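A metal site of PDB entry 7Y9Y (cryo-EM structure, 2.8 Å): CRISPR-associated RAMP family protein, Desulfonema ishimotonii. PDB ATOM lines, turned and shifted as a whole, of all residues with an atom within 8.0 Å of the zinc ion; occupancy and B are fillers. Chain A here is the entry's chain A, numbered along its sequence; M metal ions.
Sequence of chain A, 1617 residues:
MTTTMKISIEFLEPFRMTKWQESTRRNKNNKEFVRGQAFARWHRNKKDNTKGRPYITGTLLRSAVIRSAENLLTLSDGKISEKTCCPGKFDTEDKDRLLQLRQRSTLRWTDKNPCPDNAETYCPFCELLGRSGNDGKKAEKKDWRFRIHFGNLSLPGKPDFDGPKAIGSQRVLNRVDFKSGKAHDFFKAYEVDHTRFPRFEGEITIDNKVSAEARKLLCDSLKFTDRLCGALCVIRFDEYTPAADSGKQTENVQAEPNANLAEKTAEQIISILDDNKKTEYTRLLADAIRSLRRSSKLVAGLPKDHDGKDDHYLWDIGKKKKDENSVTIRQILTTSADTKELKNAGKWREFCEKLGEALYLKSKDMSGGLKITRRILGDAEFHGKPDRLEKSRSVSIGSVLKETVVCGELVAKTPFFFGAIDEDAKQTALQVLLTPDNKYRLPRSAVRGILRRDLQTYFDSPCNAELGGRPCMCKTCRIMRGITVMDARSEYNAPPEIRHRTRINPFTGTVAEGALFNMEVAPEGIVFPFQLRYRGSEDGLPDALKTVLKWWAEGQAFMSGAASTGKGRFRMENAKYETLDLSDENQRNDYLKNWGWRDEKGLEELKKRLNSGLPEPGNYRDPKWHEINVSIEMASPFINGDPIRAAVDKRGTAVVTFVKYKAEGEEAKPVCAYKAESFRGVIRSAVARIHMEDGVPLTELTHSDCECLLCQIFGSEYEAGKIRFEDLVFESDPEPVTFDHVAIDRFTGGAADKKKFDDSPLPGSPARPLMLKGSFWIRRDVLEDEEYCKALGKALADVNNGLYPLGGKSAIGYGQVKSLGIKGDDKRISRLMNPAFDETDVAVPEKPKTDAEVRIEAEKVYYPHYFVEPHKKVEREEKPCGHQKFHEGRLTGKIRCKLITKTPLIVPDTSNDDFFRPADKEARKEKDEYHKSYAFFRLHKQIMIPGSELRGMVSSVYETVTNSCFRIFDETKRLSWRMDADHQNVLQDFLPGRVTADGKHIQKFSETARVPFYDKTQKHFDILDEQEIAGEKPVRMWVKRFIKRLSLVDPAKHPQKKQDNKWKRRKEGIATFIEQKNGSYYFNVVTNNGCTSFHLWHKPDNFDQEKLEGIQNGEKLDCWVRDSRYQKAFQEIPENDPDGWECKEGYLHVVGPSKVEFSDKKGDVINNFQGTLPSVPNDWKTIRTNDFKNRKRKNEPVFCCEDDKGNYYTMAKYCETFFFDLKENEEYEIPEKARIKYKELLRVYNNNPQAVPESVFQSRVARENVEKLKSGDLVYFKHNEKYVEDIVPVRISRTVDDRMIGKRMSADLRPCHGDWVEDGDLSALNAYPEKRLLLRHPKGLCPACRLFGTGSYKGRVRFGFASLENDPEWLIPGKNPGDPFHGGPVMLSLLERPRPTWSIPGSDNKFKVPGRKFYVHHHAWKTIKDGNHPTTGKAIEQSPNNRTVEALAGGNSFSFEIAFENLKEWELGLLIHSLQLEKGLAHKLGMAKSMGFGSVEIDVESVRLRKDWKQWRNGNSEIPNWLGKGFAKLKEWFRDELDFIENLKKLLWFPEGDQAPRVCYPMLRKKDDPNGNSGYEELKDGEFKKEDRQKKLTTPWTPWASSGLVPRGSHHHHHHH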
ATOM      1  N   LYS A  83       4.153  14.034  14.788  1.00  0.00           N
ATOM      2  CA  LYS A  83       2.994  14.759  14.291  1.00  0.00           C
ATOM      3  C   LYS A  83       3.362  16.199  13.920  1.00  0.00           C
ATOM      4  O   LYS A  83       4.301  16.790  14.442  1.00  0.00           O
ATOM      5  CB  LYS A  83       1.878  14.766  15.338  1.00  0.00           C
ATOM      6  CG  LYS A  83       1.191  13.422  15.510  1.00  0.00           C
ATOM      7  CD  LYS A  83      -0.194  13.596  16.103  1.00  0.00           C
ATOM      8  CE  LYS A  83      -1.113  14.347  15.151  1.00  0.00           C
ATOM      9  NZ  LYS A  83      -2.492  14.484  15.695  1.00  0.00           N
ATOM     10  N   THR A  84       2.589  16.749  12.985  1.00  0.00           N
ATOM     11  CA  THR A  84       2.697  18.144  12.563  1.00  0.00           C
ATOM     12  C   THR A  84       1.484  18.917  13.072  1.00  0.00           C
ATOM     13  O   THR A  84       0.448  18.332  13.390  1.00  0.00           O
ATOM     14  CB  THR A  84       2.794  18.240  11.032  1.00  0.00           C
ATOM     15  OG1 THR A  84       3.528  17.118  10.529  1.00  0.00           O
ATOM     16  CG2 THR A  84       3.513  19.519  10.625  1.00  0.00           C
ATOM     17  N   CYS A  85       1.637  20.232  13.138  1.00  0.00           N
ATOM     18  CA  CYS A  85       0.607  21.095  13.713  1.00  0.00           C
ATOM     19  C   CYS A  85       0.128  22.107  12.691  1.00  0.00           C
ATOM     20  O   CYS A  85       0.933  22.668  11.931  1.00  0.00           O
ATOM     21  CB  CYS A  85       1.129  21.831  14.957  1.00  0.00           C
ATOM     22  SG  CYS A  85       1.573  20.751  16.331  1.00  0.00           S
ATOM     23  N   CYS A  86      -1.187  22.346  12.673  1.00  0.00           N
ATOM     24  CA  CYS A  86      -1.760  23.399  11.864  1.00  0.00           C
ATOM     25  C   CYS A  86      -1.507  24.747  12.526  1.00  0.00           C
ATOM     26  O   CYS A  86      -1.105  24.815  13.694  1.00  0.00           O
ATOM     27  CB  CYS A  86      -3.258  23.175  11.687  1.00  0.00           C
ATOM     28  SG  CYS A  86      -4.250  23.590  13.137  1.00  0.00           S
ATOM     29  N   PRO A  87      -1.721  25.858  11.804  1.00  0.00           N
ATOM     30  CA  PRO A  87      -1.506  27.181  12.415  1.00  0.00           C
ATOM     31  C   PRO A  87      -2.439  27.500  13.573  1.00  0.00           C
ATOM     32  O   PRO A  87      -2.209  28.497  14.268  1.00  0.00           O
ATOM     33  CB  PRO A  87      -1.743  28.067  11.208  1.00  0.00           C
ATOM     34  CG  PRO A  87      -2.931  27.274  10.743  1.00  0.00           C
ATOM     35  CD  PRO A  87      -2.097  26.129  10.407  1.00  0.00           C
ATOM     36  N   GLY A  88      -3.476  26.704  13.800  1.00  0.00           N
ATOM     37  CA  GLY A  88      -4.442  26.983  14.841  1.00  0.00           C
ATOM     38  C   GLY A  88      -5.505  27.977  14.401  1.00  0.00           C
ATOM     39  O   GLY A  88      -5.417  28.604  13.340  1.00  0.00           O
ATOM     40  N   LYS A  89      -6.526  28.128  15.244  1.00  0.00           N
ATOM     41  CA  LYS A  89      -7.645  28.999  14.947  1.00  0.00           C
ATOM     42  C   LYS A  89      -7.734  30.082  16.011  1.00  0.00           C
ATOM     43  O   LYS A  89      -7.771  29.778  17.208  1.00  0.00           O
ATOM     44  CB  LYS A  89      -8.961  28.225  14.871  1.00  0.00           C
ATOM     45  CG  LYS A  89     -10.197  29.105  14.817  1.00  0.00           C
ATOM     46  CD  LYS A  89     -11.411  28.318  14.365  1.00  0.00           C
ATOM     47  CE  LYS A  89     -11.327  27.965  12.889  1.00  0.00           C
ATOM     48  NZ  LYS A  89     -12.634  27.452  12.355  1.00  0.00           N
ATOM     49  N   TRP A 109       4.141  28.897  11.031  1.00  0.00           N
ATOM     50  CA  TRP A 109       5.136  27.891  10.675  1.00  0.00           C
ATOM     51  C   TRP A 109       4.765  27.161   9.388  1.00  0.00           C
ATOM     52  O   TRP A 109       5.592  26.990   8.503  1.00  0.00           O
ATOM     53  CB  TRP A 109       5.334  26.882  11.818  1.00  0.00           C
ATOM     54  CG  TRP A 109       4.075  26.472  12.523  1.00  0.00           C
ATOM     55  CD1 TRP A 109       3.295  25.398  12.220  1.00  0.00           C
ATOM     56  CD2 TRP A 109       3.477  27.081  13.668  1.00  0.00           C
ATOM     57  NE1 TRP A 109       2.235  25.312  13.087  1.00  0.00           N
ATOM     58  CE2 TRP A 109       2.328  26.345  13.994  1.00  0.00           C
ATOM     59  CE3 TRP A 109       3.799  28.197  14.447  1.00  0.00           C
ATOM     60  CZ2 TRP A 109       1.494  26.678  15.061  1.00  0.00           C
ATOM     61  CZ3 TRP A 109       2.979  28.524  15.504  1.00  0.00           C
ATOM     62  CH2 TRP A 109       1.839  27.770  15.804  1.00  0.00           C
ATOM     63  N   LYS A 112      -0.815  25.131   5.700  1.00  0.00           N
ATOM     64  CA  LYS A 112      -2.074  24.450   5.454  1.00  0.00           C
ATOM     65  C   LYS A 112      -3.159  25.023   6.350  1.00  0.00           C
ATOM     66  O   LYS A 112      -2.895  25.707   7.333  1.00  0.00           O
ATOM     67  CB  LYS A 112      -1.973  22.927   5.671  1.00  0.00           C
ATOM     68  CG  LYS A 112      -2.070  22.441   7.110  1.00  0.00           C
ATOM     69  CD  LYS A 112      -0.948  21.485   7.472  1.00  0.00           C
ATOM     70  CE  LYS A 112       0.299  22.212   7.863  1.00  0.00           C
ATOM     71  NZ  LYS A 112       1.398  21.298   8.260  1.00  0.00           N
ATOM     72  N   ASN A 113      -4.410  24.748   5.981  1.00  0.00           N
ATOM     73  CA  ASN A 113      -5.553  25.286   6.698  1.00  0.00           C
ATOM     74  C   ASN A 113      -5.657  24.676   8.092  1.00  0.00           C
ATOM     75  O   ASN A 113      -5.133  23.591   8.347  1.00  0.00           O
ATOM     76  CB  ASN A 113      -6.829  25.035   5.917  1.00  0.00           C
ATOM     77  CG  ASN A 113      -7.150  26.148   4.944  1.00  0.00           C
ATOM     78  OD1 ASN A 113      -6.739  27.296   5.135  1.00  0.00           O
ATOM     79  ND2 ASN A 113      -7.891  25.822   3.890  1.00  0.00           N
ATOM     80  N   PRO A 114      -6.320  25.364   9.021  1.00  0.00           N
ATOM     81  CA  PRO A 114      -6.505  24.810  10.361  1.00  0.00           C
ATOM     82  C   PRO A 114      -7.310  23.521  10.344  1.00  0.00           C
ATOM     83  O   PRO A 114      -7.941  23.163   9.348  1.00  0.00           O
ATOM     84  CB  PRO A 114      -7.250  25.923  11.102  1.00  0.00           C
ATOM     85  CG  PRO A 114      -6.878  27.170  10.369  1.00  0.00           C
ATOM     86  CD  PRO A 114      -6.788  26.755   8.928  1.00  0.00           C
ATOM     87  N   CYS A 115      -7.279  22.828  11.474  1.00  0.00           N
ATOM     88  CA  CYS A 115      -8.014  21.581  11.617  1.00  0.00           C
ATOM     89  C   CYS A 115      -9.514  21.836  11.439  1.00  0.00           C
ATOM     90  O   CYS A 115     -10.014  22.914  11.797  1.00  0.00           O
ATOM     91  CB  CYS A 115      -7.750  20.944  12.984  1.00  0.00           C
ATOM     92  SG  CYS A 115      -6.059  20.352  13.238  1.00  0.00           S
ATOM     93  N   PRO A 116     -10.238  20.875  10.875  1.00  0.00           N
ATOM     94  CA  PRO A 116     -11.683  21.066  10.673  1.00  0.00           C
ATOM     95  C   PRO A 116     -12.396  21.310  11.992  1.00  0.00           C
ATOM     96  O   PRO A 116     -12.014  20.784  13.037  1.00  0.00           O
ATOM     97  CB  PRO A 116     -12.119  19.746  10.033  1.00  0.00           C
ATOM     98  CG  PRO A 116     -10.888  19.216   9.371  1.00  0.00           C
ATOM     99  CD  PRO A 116      -9.758  19.631  10.265  1.00  0.00           C
ATOM    100  N   THR A 121      -9.715  13.516  14.543  1.00  0.00           N
ATOM    101  CA  THR A 121      -8.350  13.692  14.996  1.00  0.00           C
ATOM    102  C   THR A 121      -7.968  15.171  14.924  1.00  0.00           C
ATOM    103  O   THR A 121      -8.228  15.838  13.928  1.00  0.00           O
ATOM    104  CB  THR A 121      -7.371  12.877  14.151  1.00  0.00           C
ATOM    105  OG1 THR A 121      -7.358  13.372  12.810  1.00  0.00           O
ATOM    106  CG2 THR A 121      -7.789  11.406  14.135  1.00  0.00           C
ATOM    107  N   TYR A 122      -7.346  15.664  15.995  1.00  0.00           N
ATOM    108  CA  TYR A 122      -6.897  17.033  16.072  1.00  0.00           C
ATOM    109  C   TYR A 122      -5.385  17.063  16.284  1.00  0.00           C
ATOM    110  O   TYR A 122      -4.816  16.189  16.942  1.00  0.00           O
ATOM    111  CB  TYR A 122      -7.581  17.792  17.218  1.00  0.00           C
ATOM    112  CG  TYR A 122      -8.867  18.486  16.819  1.00  0.00           C
ATOM    113  CD1 TYR A 122     -10.039  17.772  16.622  1.00  0.00           C
ATOM    114  CD2 TYR A 122      -8.903  19.860  16.654  1.00  0.00           C
ATOM    115  CE1 TYR A 122     -11.203  18.404  16.262  1.00  0.00           C
ATOM    116  CE2 TYR A 122     -10.073  20.504  16.299  1.00  0.00           C
ATOM    117  CZ  TYR A 122     -11.222  19.773  16.111  1.00  0.00           C
ATOM    118  OH  TYR A 122     -12.386  20.405  15.751  1.00  0.00           O
ATOM    119  N   CYS A 123      -4.743  18.075  15.713  1.00  0.00           N
ATOM    120  CA  CYS A 123      -3.309  18.241  15.882  1.00  0.00           C
ATOM    121  C   CYS A 123      -2.998  18.618  17.324  1.00  0.00           C
ATOM    122  O   CYS A 123      -3.855  19.152  18.035  1.00  0.00           O
ATOM    123  CB  CYS A 123      -2.784  19.301  14.911  1.00  0.00           C
ATOM    124  SG  CYS A 123      -2.870  20.992  15.517  1.00  0.00           S
ATOM    125  N   PRO A 124      -1.779  18.337  17.798  1.00  0.00           N
ATOM    126  CA  PRO A 124      -1.452  18.609  19.204  1.00  0.00           C
ATOM    127  C   PRO A 124      -1.624  20.066  19.597  1.00  0.00           C
ATOM    128  O   PRO A 124      -1.977  20.342  20.755  1.00  0.00           O
ATOM    129  CB  PRO A 124       0.013  18.178  19.307  1.00  0.00           C
ATOM    130  CG  PRO A 124       0.162  17.130  18.257  1.00  0.00           C
ATOM    131  CD  PRO A 124      -0.681  17.615  17.116  1.00  0.00           C
ATOM    132  N   PHE A 125      -1.390  21.012  18.686  1.00  0.00           N
ATOM    133  CA  PHE A 125      -1.564  22.415  19.020  1.00  0.00           C
ATOM    134  C   PHE A 125      -3.022  22.733  19.309  1.00  0.00           C
ATOM    135  O   PHE A 125      -3.334  23.570  20.154  1.00  0.00           O
ATOM    136  CB  PHE A 125      -1.015  23.297  17.889  1.00  0.00           C
ATOM    137  CG  PHE A 125      -1.084  24.762  18.170  1.00  0.00           C
ATOM    138  CD1 PHE A 125      -0.191  25.349  19.060  1.00  0.00           C
ATOM    139  CD2 PHE A 125      -1.995  25.565  17.521  1.00  0.00           C
ATOM    140  CE1 PHE A 125      -0.242  26.704  19.320  1.00  0.00           C
ATOM    141  CE2 PHE A 125      -2.040  26.925  17.777  1.00  0.00           C
ATOM    142  CZ  PHE A 125      -1.167  27.489  18.675  1.00  0.00           C
ATOM    143  N   CYS A 126      -3.941  22.055  18.609  1.00  0.00           N
ATOM    144  CA  CYS A 126      -5.365  22.252  18.884  1.00  0.00           C
ATOM    145  C   CYS A 126      -5.769  21.614  20.196  1.00  0.00           C
ATOM    146  O   CYS A 126      -6.616  22.155  20.926  1.00  0.00           O
ATOM    147  CB  CYS A 126      -6.194  21.696  17.729  1.00  0.00           C
ATOM    148  SG  CYS A 126      -6.150  22.700  16.231  1.00  0.00           S
ATOM    149  N   GLU A 127      -5.189  20.458  20.536  1.00  0.00           N
ATOM    150  CA  GLU A 127      -5.459  19.855  21.837  1.00  0.00           C
ATOM    151  C   GLU A 127      -4.979  20.754  22.962  1.00  0.00           C
ATOM    152  O   GLU A 127      -5.654  20.890  23.989  1.00  0.00           O
ATOM    153  CB  GLU A 127      -4.803  18.477  21.941  1.00  0.00           C
ATOM    154  CG  GLU A 127      -5.071  17.555  20.760  1.00  0.00           C
ATOM    155  CD  GLU A 127      -4.589  16.146  21.018  1.00  0.00           C
ATOM    156  OE1 GLU A 127      -4.969  15.568  22.051  1.00  0.00           O
ATOM    157  OE2 GLU A 127      -3.825  15.613  20.182  1.00  0.00           O
ATOM    158  N   LEU A 129      -4.733  23.997  22.644  1.00  0.00           N
ATOM    159  CA  LEU A 129      -5.680  25.098  22.600  1.00  0.00           C
ATOM    160  C   LEU A 129      -6.981  24.739  23.310  1.00  0.00           C
ATOM    161  O   LEU A 129      -7.561  25.575  24.009  1.00  0.00           O
ATOM    162  CB  LEU A 129      -5.965  25.483  21.150  1.00  0.00           C
ATOM    163  CG  LEU A 129      -5.002  26.429  20.437  1.00  0.00           C
ATOM    164  CD1 LEU A 129      -5.362  26.518  18.962  1.00  0.00           C
ATOM    165  CD2 LEU A 129      -5.042  27.803  21.064  1.00  0.00           C
ATOM    166  N   ARG A 131      -9.485  22.862  21.352  1.00  0.00           N
ATOM    167  CA  ARG A 131     -10.502  22.667  20.320  1.00  0.00           C
ATOM    168  C   ARG A 131     -11.132  21.286  20.409  1.00  0.00           C
ATOM    169  O   ARG A 131     -12.350  21.144  20.236  1.00  0.00           O
ATOM    170  CB  ARG A 131      -9.894  22.888  18.939  1.00  0.00           C
ATOM    171  CG  ARG A 131      -8.931  24.059  18.868  1.00  0.00           C
ATOM    172  CD  ARG A 131      -9.505  25.216  18.055  1.00  0.00           C
ATOM    173  NE  ARG A 131     -10.340  24.755  16.956  1.00  0.00           N
ATOM    174  CZ  ARG A 131      -9.882  24.346  15.781  1.00  0.00           C
ATOM    175  NH1 ARG A 131      -8.587  24.333  15.512  1.00  0.00           N
ATOM    176  NH2 ARG A 131     -10.747  23.954  14.850  1.00  0.00           N
HETATM  177 ZN    ZN M   1      -4.819  21.834  14.539  1.00  0.00          ZN
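The backbone NH (N) of Phe 125 lies close to the side-chain sulfur (SG) of Cys 123 (3.5 Å). The backbone NH (N) of Arg 131 lies within hydrogen-bond range of the backbone carbonyl oxygen (O) of Cys 126. The backbone carbonyl oxygen (O) of Cys 86 sits at hydrogen-bond distance from the indole nitrogen (NE1) of Trp 109. O of Cys 115 sits at hydrogen-bond distance from NH2 of Arg 131 (3.3 Å). The side-chain sulfur of Cys 86 lies close to the backbone NH of Gly 88 (3.3 Å).
Within 4 Å of the zinc ion: Cys 86, Cys 115, Cys 123 and Cys 126.
The zinc ion is bound by SG of Cys 86 (2.3 Å). The zinc ion is bound by the side-chain sulfur (SG) of Cys 126 (2.3 Å). The zinc ion is bound by SG of Cys 115, at 2.3 Å. SG of Cys 123 is bound to the zinc ion. The zinc ion has four donor atoms within binding distance.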
